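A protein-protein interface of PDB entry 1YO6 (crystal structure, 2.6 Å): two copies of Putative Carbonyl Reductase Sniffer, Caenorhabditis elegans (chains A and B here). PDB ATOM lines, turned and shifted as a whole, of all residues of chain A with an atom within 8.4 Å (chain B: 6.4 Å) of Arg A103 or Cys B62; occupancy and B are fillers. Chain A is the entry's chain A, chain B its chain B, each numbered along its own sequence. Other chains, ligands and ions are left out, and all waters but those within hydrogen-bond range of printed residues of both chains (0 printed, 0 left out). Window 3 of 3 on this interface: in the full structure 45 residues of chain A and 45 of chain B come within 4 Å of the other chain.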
ATOM      1  N   TYR A  95      24.014 -13.192 -26.899  1.00  0.00           N
ATOM      2  CA  TYR A  95      24.386 -11.826 -27.273  1.00  0.00           C
ATOM      3  C   TYR A  95      25.503 -11.780 -28.310  1.00  0.00           C
ATOM      4  O   TYR A  95      26.621 -12.224 -28.068  1.00  0.00           O
ATOM      5  CB  TYR A  95      24.800 -11.019 -26.033  1.00  0.00           C
ATOM      6  CG  TYR A  95      24.803  -9.509 -26.244  1.00  0.00           C
ATOM      7  CD1 TYR A  95      25.897  -8.858 -26.816  1.00  0.00           C
ATOM      8  CD2 TYR A  95      23.717  -8.732 -25.849  1.00  0.00           C
ATOM      9  CE1 TYR A  95      25.914  -7.481 -26.979  1.00  0.00           C
ATOM     10  CE2 TYR A  95      23.722  -7.344 -26.012  1.00  0.00           C
ATOM     11  CZ  TYR A  95      24.826  -6.727 -26.573  1.00  0.00           C
ATOM     12  OH  TYR A  95      24.847  -5.352 -26.684  1.00  0.00           O
ATOM     13  N   GLU A 100      20.191  -6.297 -30.314  1.00  0.00           N
ATOM     14  CA  GLU A 100      19.804  -4.959 -29.880  1.00  0.00           C
ATOM     15  C   GLU A 100      20.782  -4.630 -28.747  1.00  0.00           C
ATOM     16  O   GLU A 100      20.836  -5.340 -27.742  1.00  0.00           O
ATOM     17  CB  GLU A 100      18.401  -5.000 -29.361  1.00  0.00           C
ATOM     18  CG  GLU A 100      17.879  -3.595 -29.035  1.00  0.00           C
ATOM     19  CD  GLU A 100      17.652  -2.832 -30.320  1.00  0.00           C
ATOM     20  OE1 GLU A 100      17.641  -3.450 -31.375  1.00  0.00           O
ATOM     21  OE2 GLU A 100      17.487  -1.615 -30.254  1.00  0.00           O
ATOM     22  N   PRO A 101      21.605  -3.579 -28.921  1.00  0.00           N
ATOM     23  CA  PRO A 101      22.567  -3.222 -27.875  1.00  0.00           C
ATOM     24  C   PRO A 101      21.895  -3.295 -26.522  1.00  0.00           C
ATOM     25  O   PRO A 101      20.848  -2.690 -26.329  1.00  0.00           O
ATOM     26  CB  PRO A 101      22.967  -1.797 -28.244  1.00  0.00           C
ATOM     27  CG  PRO A 101      22.892  -1.811 -29.732  1.00  0.00           C
ATOM     28  CD  PRO A 101      21.601  -2.571 -29.997  1.00  0.00           C
ATOM     29  N   ASN A 102      22.483  -4.047 -25.596  1.00  0.00           N
ATOM     30  CA  ASN A 102      21.917  -4.180 -24.258  1.00  0.00           C
ATOM     31  C   ASN A 102      23.005  -4.292 -23.189  1.00  0.00           C
ATOM     32  O   ASN A 102      23.661  -5.334 -23.054  1.00  0.00           O
ATOM     33  CB  ASN A 102      21.012  -5.401 -24.202  1.00  0.00           C
ATOM     34  CG  ASN A 102      20.171  -5.427 -22.958  1.00  0.00           C
ATOM     35  OD1 ASN A 102      20.688  -5.475 -21.836  1.00  0.00           O
ATOM     36  ND2 ASN A 102      18.857  -5.387 -23.143  1.00  0.00           N
ATOM     37  N   ARG A 103      23.181  -3.228 -22.418  1.00  0.00           N
ATOM     38  CA  ARG A 103      24.211  -3.217 -21.398  1.00  0.00           C
ATOM     39  C   ARG A 103      24.023  -4.245 -20.289  1.00  0.00           C
ATOM     40  O   ARG A 103      24.989  -4.877 -19.868  1.00  0.00           O
ATOM     41  CB  ARG A 103      24.334  -1.815 -20.791  1.00  0.00           C
ATOM     42  CG  ARG A 103      25.516  -1.652 -19.848  1.00  0.00           C
ATOM     43  CD  ARG A 103      25.496  -0.276 -19.199  1.00  0.00           C
ATOM     44  NE  ARG A 103      25.691   0.798 -20.172  1.00  0.00           N
ATOM     45  CZ  ARG A 103      26.879   1.226 -20.574  1.00  0.00           C
ATOM     46  NH1 ARG A 103      27.980   0.680 -20.082  1.00  0.00           N
ATOM     47  NH2 ARG A 103      26.965   2.190 -21.474  1.00  0.00           N
ATOM     48  N   ALA A 104      22.790  -4.420 -19.819  1.00  0.00           N
ATOM     49  CA  ALA A 104      22.511  -5.365 -18.734  1.00  0.00           C
ATOM     50  C   ALA A 104      22.916  -6.794 -19.081  1.00  0.00           C
ATOM     51  O   ALA A 104      23.439  -7.517 -18.240  1.00  0.00           O
ATOM     52  CB  ALA A 104      21.037  -5.321 -18.359  1.00  0.00           C
ATOM     53  N   VAL A 105      22.680  -7.207 -20.320  1.00  0.00           N
ATOM     54  CA  VAL A 105      23.057  -8.554 -20.704  1.00  0.00           C
ATOM     55  C   VAL A 105      24.578  -8.704 -20.761  1.00  0.00           C
ATOM     56  O   VAL A 105      25.129  -9.642 -20.188  1.00  0.00           O
ATOM     57  CB  VAL A 105      22.432  -8.946 -22.050  1.00  0.00           C
ATOM     58  CG1 VAL A 105      22.889 -10.342 -22.448  1.00  0.00           C
ATOM     59  CG2 VAL A 105      20.910  -8.898 -21.937  1.00  0.00           C
ATOM     60  N   ILE A 106      25.267  -7.786 -21.431  1.00  0.00           N
ATOM     61  CA  ILE A 106      26.718  -7.876 -21.498  1.00  0.00           C
ATOM     62  C   ILE A 106      27.286  -7.900 -20.070  1.00  0.00           C
ATOM     63  O   ILE A 106      28.146  -8.731 -19.743  1.00  0.00           O
ATOM     64  CB  ILE A 106      27.324  -6.686 -22.270  1.00  0.00           C
ATOM     65  CG1 ILE A 106      26.831  -6.702 -23.715  1.00  0.00           C
ATOM     66  CG2 ILE A 106      28.831  -6.764 -22.246  1.00  0.00           C
ATOM     67  CD1 ILE A 106      27.228  -5.472 -24.514  1.00  0.00           C
ATOM     68  N   ALA A 107      26.783  -7.002 -19.224  1.00  0.00           N
ATOM     69  CA  ALA A 107      27.236  -6.910 -17.836  1.00  0.00           C
ATOM     70  C   ALA A 107      26.992  -8.183 -17.007  1.00  0.00           C
ATOM     71  O   ALA A 107      27.793  -8.508 -16.117  1.00  0.00           O
ATOM     72  CB  ALA A 107      26.579  -5.708 -17.141  1.00  0.00           C
ATOM     73  N   GLU A 108      25.905  -8.904 -17.291  1.00  0.00           N
ATOM     74  CA  GLU A 108      25.601 -10.122 -16.540  1.00  0.00           C
ATOM     75  C   GLU A 108      26.526 -11.259 -16.951  1.00  0.00           C
ATOM     76  O   GLU A 108      26.954 -12.063 -16.119  1.00  0.00           O
ATOM     77  CB  GLU A 108      24.152 -10.556 -16.763  1.00  0.00           C
ATOM     78  CG  GLU A 108      23.595 -11.386 -15.604  1.00  0.00           C
ATOM     79  CD  GLU A 108      22.317 -12.134 -15.953  1.00  0.00           C
ATOM     80  OE1 GLU A 108      21.440 -11.554 -16.630  1.00  0.00           O
ATOM     81  OE2 GLU A 108      22.185 -13.304 -15.535  1.00  0.00           O
ATOM     82  N   GLN A 109      26.827 -11.307 -18.243  1.00  0.00           N
ATOM     83  CA  GLN A 109      27.685 -12.328 -18.810  1.00  0.00           C
ATOM     84  C   GLN A 109      29.064 -12.242 -18.181  1.00  0.00           C
ATOM     85  O   GLN A 109      29.659 -13.273 -17.838  1.00  0.00           O
ATOM     86  CB  GLN A 109      27.785 -12.132 -20.320  1.00  0.00           C
ATOM     87  CG  GLN A 109      28.564 -13.193 -21.059  1.00  0.00           C
ATOM     88  CD  GLN A 109      28.040 -14.594 -20.802  1.00  0.00           C
ATOM     89  OE1 GLN A 109      28.194 -15.133 -19.700  1.00  0.00           O
ATOM     90  NE2 GLN A 109      27.413 -15.191 -21.814  1.00  0.00           N
ATOM     91  N   LEU A 110      29.560 -11.015 -18.021  1.00  0.00           N
ATOM     92  CA  LEU A 110      30.881 -10.778 -17.433  1.00  0.00           C
ATOM     93  C   LEU A 110      30.873 -10.979 -15.917  1.00  0.00           C
ATOM     94  O   LEU A 110      31.790 -11.567 -15.352  1.00  0.00           O
ATOM     95  CB  LEU A 110      31.357  -9.361 -17.773  1.00  0.00           C
ATOM     96  CG  LEU A 110      31.622  -9.094 -19.263  1.00  0.00           C
ATOM     97  CD1 LEU A 110      31.772  -7.616 -19.519  1.00  0.00           C
ATOM     98  CD2 LEU A 110      32.875  -9.831 -19.696  1.00  0.00           C
ATOM     99  N   ALA A 171      29.464 -11.694 -26.052  1.00  0.00           N
ATOM    100  CA  ALA A 171      29.669 -11.436 -24.630  1.00  0.00           C
ATOM    101  C   ALA A 171      30.346 -12.613 -23.982  1.00  0.00           C
ATOM    102  O   ALA A 171      31.309 -12.457 -23.250  1.00  0.00           O
ATOM    103  CB  ALA A 171      28.347 -11.166 -23.949  1.00  0.00           C
ATOM    104  N   LEU B  58      29.853  13.186 -24.108  1.00  0.00           N
ATOM    105  CA  LEU B  58      29.555  11.761 -24.094  1.00  0.00           C
ATOM    106  C   LEU B  58      30.165  11.079 -22.885  1.00  0.00           C
ATOM    107  O   LEU B  58      31.356  11.203 -22.624  1.00  0.00           O
ATOM    108  CB  LEU B  58      30.071  11.074 -25.362  1.00  0.00           C
ATOM    109  CG  LEU B  58      30.085   9.538 -25.268  1.00  0.00           C
ATOM    110  CD1 LEU B  58      28.668   8.999 -25.214  1.00  0.00           C
ATOM    111  CD2 LEU B  58      30.820   8.957 -26.441  1.00  0.00           C
ATOM    112  N   THR B  59      29.334  10.364 -22.143  1.00  0.00           N
ATOM    113  CA  THR B  59      29.802   9.637 -20.976  1.00  0.00           C
ATOM    114  C   THR B  59      29.492   8.150 -21.215  1.00  0.00           C
ATOM    115  O   THR B  59      28.422   7.657 -20.862  1.00  0.00           O
ATOM    116  CB  THR B  59      29.124  10.171 -19.683  1.00  0.00           C
ATOM    117  OG1 THR B  59      29.257   9.207 -18.630  1.00  0.00           O
ATOM    118  CG2 THR B  59      27.666  10.470 -19.929  1.00  0.00           C
ATOM    119  N   VAL B  60      30.456   7.472 -21.839  1.00  0.00           N
ATOM    120  CA  VAL B  60      30.397   6.058 -22.222  1.00  0.00           C
ATOM    121  C   VAL B  60      29.576   5.058 -21.403  1.00  0.00           C
ATOM    122  O   VAL B  60      29.032   4.100 -21.964  1.00  0.00           O
ATOM    123  CB  VAL B  60      31.810   5.489 -22.349  1.00  0.00           C
ATOM    124  CG1 VAL B  60      32.649   6.396 -23.235  1.00  0.00           C
ATOM    125  CG2 VAL B  60      32.428   5.334 -20.976  1.00  0.00           C
ATOM    126  N   THR B  61      29.482   5.260 -20.094  1.00  0.00           N
ATOM    127  CA  THR B  61      28.731   4.346 -19.242  1.00  0.00           C
ATOM    128  C   THR B  61      27.220   4.623 -19.171  1.00  0.00           C
ATOM    129  O   THR B  61      26.465   3.854 -18.573  1.00  0.00           O
ATOM    130  CB  THR B  61      29.308   4.368 -17.823  1.00  0.00           C
ATOM    131  OG1 THR B  61      29.480   5.727 -17.414  1.00  0.00           O
ATOM    132  CG2 THR B  61      30.658   3.671 -17.775  1.00  0.00           C
ATOM    133  N   CYS B  62      26.777   5.713 -19.789  1.00  0.00           N
ATOM    134  CA  CYS B  62      25.365   6.098 -19.774  1.00  0.00           C
ATOM    135  C   CYS B  62      24.710   5.874 -21.136  1.00  0.00           C
ATOM    136  O   CYS B  62      25.094   6.499 -22.130  1.00  0.00           O
ATOM    137  CB  CYS B  62      25.236   7.573 -19.367  1.00  0.00           C
ATOM    138  SG  CYS B  62      23.565   8.256 -19.495  1.00  0.00           S
ATOM    139  N   ASP B  63      23.713   4.993 -21.173  1.00  0.00           N
ATOM    140  CA  ASP B  63      23.028   4.670 -22.419  1.00  0.00           C
ATOM    141  C   ASP B  63      22.286   5.859 -23.058  1.00  0.00           C
ATOM    142  O   ASP B  63      22.141   5.930 -24.285  1.00  0.00           O
ATOM    143  CB  ASP B  63      22.085   3.480 -22.192  1.00  0.00           C
ATOM    144  CG  ASP B  63      22.810   2.265 -21.608  1.00  0.00           C
ATOM    145  OD1 ASP B  63      23.899   1.921 -22.122  1.00  0.00           O
ATOM    146  OD2 ASP B  63      22.298   1.652 -20.636  1.00  0.00           O
ATOM    147  N   LYS B  64      21.817   6.793 -22.240  1.00  0.00           N
ATOM    148  CA  LYS B  64      21.137   7.959 -22.790  1.00  0.00           C
ATOM    149  C   LYS B  64      22.185   8.869 -23.415  1.00  0.00           C
ATOM    150  O   LYS B  64      21.972   9.441 -24.484  1.00  0.00           O
ATOM    151  CB  LYS B  64      20.344   8.694 -21.702  1.00  0.00           C
ATOM    152  CG  LYS B  64      19.089   7.923 -21.288  1.00  0.00           C
ATOM    153  CD  LYS B  64      18.198   7.625 -22.512  1.00  0.00           C
ATOM    154  CE  LYS B  64      17.314   6.380 -22.324  1.00  0.00           C
ATOM    155  NZ  LYS B  64      16.312   6.496 -21.224  1.00  0.00           N
ATOM    156  N   SER B  65      23.335   8.977 -22.760  1.00  0.00           N
ATOM    157  CA  SER B  65      24.410   9.805 -23.283  1.00  0.00           C
ATOM    158  C   SER B  65      24.948   9.172 -24.552  1.00  0.00           C
ATOM    159  O   SER B  65      25.441   9.874 -25.427  1.00  0.00           O
ATOM    160  CB  SER B  65      25.534   9.952 -22.258  1.00  0.00           C
ATOM    161  OG  SER B  65      26.588  10.740 -22.784  1.00  0.00           O
ATOM    162  N   LEU B  66      24.851   7.845 -24.647  1.00  0.00           N
ATOM    163  CA  LEU B  66      25.308   7.125 -25.837  1.00  0.00           C
ATOM    164  C   LEU B  66      24.400   7.426 -27.027  1.00  0.00           C
ATOM    165  O   LEU B  66      24.875   7.897 -28.065  1.00  0.00           O
ATOM    166  CB  LEU B  66      25.336   5.608 -25.595  1.00  0.00           C
ATOM    167  CG  LEU B  66      26.631   4.952 -25.106  1.00  0.00           C
ATOM    168  CD1 LEU B  66      26.438   3.443 -25.006  1.00  0.00           C
ATOM    169  CD2 LEU B  66      27.760   5.265 -26.067  1.00  0.00           C
ATOM    170  N   ASP B  67      23.101   7.167 -26.870  1.00  0.00           N
ATOM    171  CA  ASP B  67      22.128   7.413 -27.940  1.00  0.00           C
ATOM    172  C   ASP B  67      22.175   8.853 -28.435  1.00  0.00           C
ATOM    173  O   ASP B  67      22.327   9.103 -29.630  1.00  0.00           O
ATOM    174  CB  ASP B  67      20.703   7.099 -27.470  1.00  0.00           C
ATOM    175  CG  ASP B  67      20.507   5.633 -27.138  1.00  0.00           C
ATOM    176  OD1 ASP B  67      21.342   4.815 -27.569  1.00  0.00           O
ATOM    177  OD2 ASP B  67      19.514   5.297 -26.459  1.00  0.00           O
ATOM    178  N   ASP B 111      33.137  -2.445 -17.340  1.00  0.00           N
ATOM    179  CA  ASP B 111      32.041  -1.652 -17.850  1.00  0.00           C
ATOM    180  C   ASP B 111      32.526  -0.489 -18.707  1.00  0.00           C
ATOM    181  O   ASP B 111      31.869  -0.089 -19.666  1.00  0.00           O
ATOM    182  CB  ASP B 111      31.181  -1.126 -16.710  1.00  0.00           C
ATOM    183  CG  ASP B 111      29.890  -0.496 -17.211  1.00  0.00           C
ATOM    184  OD1 ASP B 111      29.135  -1.176 -17.955  1.00  0.00           O
ATOM    185  OD2 ASP B 111      29.634   0.679 -16.869  1.00  0.00           O
ATOM    186  N   VAL B 112      33.684   0.052 -18.365  1.00  0.00           N
ATOM    187  CA  VAL B 112      34.221   1.167 -19.114  1.00  0.00           C
ATOM    188  C   VAL B 112      35.054   0.725 -20.309  1.00  0.00           C
ATOM    189  O   VAL B 112      34.867   1.219 -21.421  1.00  0.00           O
ATOM    190  CB  VAL B 112      35.098   2.075 -18.211  1.00  0.00           C
ATOM    191  CG1 VAL B 112      35.906   3.034 -19.071  1.00  0.00           C
ATOM    192  CG2 VAL B 112      34.215   2.842 -17.209  1.00  0.00           C
ATOM    193  N   THR B 115      32.297  -3.495 -22.153  1.00  0.00           N
ATOM    194  CA  THR B 115      30.900  -3.283 -22.484  1.00  0.00           C
ATOM    195  C   THR B 115      30.549  -1.897 -23.030  1.00  0.00           C
ATOM    196  O   THR B 115      29.806  -1.787 -24.010  1.00  0.00           O
ATOM    197  CB  THR B 115      30.010  -3.653 -21.271  1.00  0.00           C
ATOM    198  OG1 THR B 115      28.811  -2.868 -21.279  1.00  0.00           O
ATOM    199  CG2 THR B 115      30.763  -3.469 -19.995  1.00  0.00           C
ATOM    200  N   SER B 116      31.081  -0.839 -22.437  1.00  0.00           N
ATOM    201  CA  SER B 116      30.768   0.489 -22.948  1.00  0.00           C
ATOM    202  C   SER B 116      31.226   0.649 -24.400  1.00  0.00           C
ATOM    203  O   SER B 116      30.502   1.214 -25.225  1.00  0.00           O
ATOM    204  CB  SER B 116      31.402   1.577 -22.073  1.00  0.00           C
ATOM    205  OG  SER B 116      30.695   1.722 -20.848  1.00  0.00           O
ATOM    206  N   LEU B 119      28.979  -1.452 -26.818  1.00  0.00           N
ATOM    207  CA  LEU B 119      27.722  -0.733 -26.983  1.00  0.00           C
ATOM    208  C   LEU B 119      27.846   0.437 -27.976  1.00  0.00           C
ATOM    209  O   LEU B 119      27.062   0.551 -28.921  1.00  0.00           O
ATOM    210  CB  LEU B 119      27.248  -0.232 -25.614  1.00  0.00           C
ATOM    211  CG  LEU B 119      26.037  -0.862 -24.903  1.00  0.00           C
ATOM    212  CD1 LEU B 119      25.863  -2.309 -25.256  1.00  0.00           C
ATOM    213  CD2 LEU B 119      26.221  -0.695 -23.399  1.00  0.00           C
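The guanidinium group (NH2) of Arg A103 lies within hydrogen-bond range of the backbone carbonyl oxygen (O) of Val B60, 2.9 Å away.
The backbone carbonyl oxygen of Thr B61 lies close to the guanidinium group of Arg A103 (3.4 Å).
NE of Arg A103 lies within salt-bridge range of OD1 of Asp B63.
The guanidinium group of Arg A103 lies within salt-bridge range of the side-chain carboxylate of Asp B111.
NH1 of Arg A103 is in hydrogen-bond range of OG of Ser B116, at 3.0 Å.
The side-chain hydroxyl of Tyr A95 sits at hydrogen-bond distance from the backbone NH of Asn A102 (2.9 Å).
The side-chain amide oxygen of Asn A102 lies within hydrogen-bond range of the backbone NH of Ala A104 (3.1 Å).
The side-chain amide oxygen (OD1) of Asn A102 lies within hydrogen-bond range of the backbone NH (N) of Val A105, 3.0 Å away.
O of Val B60 sits at hydrogen-bond distance from OG of Ser B116.
The side-chain sulfur of Cys B62 sits close to the backbone NH of Lys B64 (3.6 Å).
O of Asp B111 lies within hydrogen-bond range of OG of Ser B116 (2.5 Å).
Among the printed residues, merely in contact across the chains: Arg A103 with Leu B119 (3.4 Å), Ile A106 with Thr B115 (3.5 Å), Tyr A95 with Leu B119 (3.5 Å), Ile A106 with Leu B119 (3.5 Å), Arg A103 with Leu B66 (3.8 Å), Arg A103 with Thr B115 (3.8 Å), Asn A102 with Leu B119 (3.8 Å) and Arg A103 with Cys B62 (3.9 Å).
Of chain B, only Val B60 (2.9 Å), Thr B61 (3.3 Å), Cys B62 (3.9 Å), Asp B63 (2.9 Å), Leu B66 (3.8 Å), Asp B111 (3.1 Å), Thr B115 (3.8 Å), Ser B116 (3.0 Å) and Leu B119 (3.4 Å) come within 4 Å of Arg A103.
Asp B63 touches one residue of chain A.
Of the printed residues of chain A, Thr B61 touches Arg A103.
Printed residues of chain A within 4 Å of Thr B115: Arg A103 and Ile A106.
Printed residues of chain A within 4 Å of Asp B111: Arg A103 (3.1 Å).
Asp B67 touches none of the printed residues of chain A.
The nearest residue of chain B that does not touch Arg A103 is Thr B59 (5.7 Å).
The nearest printed residue of chain A that does not touch Cys B62 is Asn A102 (10.5 Å).
Of the 15 printed residues of chain B, 9 touch a printed residue of chain A.
Hydrophobic or aromatic side chains of chain B within 4 Å of the printed part of chain A: Leu B66 and Leu B119.
Along chain B the printed residues that touch a printed residue of chain A span positions 60 to 119.
Of the 13 printed residues of chain A, 4 touch a printed residue of chain B.
Hydrophobic or aromatic side chains of chain A within 4 Å of the printed part of chain B: Tyr A95 and Ile A106.
Among the printed residues, 13 pairs touch across the chains.
Among the printed residues, Asp or Glu carboxylates within 4 Å of a Lys or Arg side-chain nitrogen of the other chain: Arg A103 with Asp B63 (2.9 Å) and Arg A103 with Asp B111 (3.1 Å).
No position is printed for both chains.
Of the 13 pairs that touch across the chains among the printed residues, none has its exchanged pair printed and touching as well.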
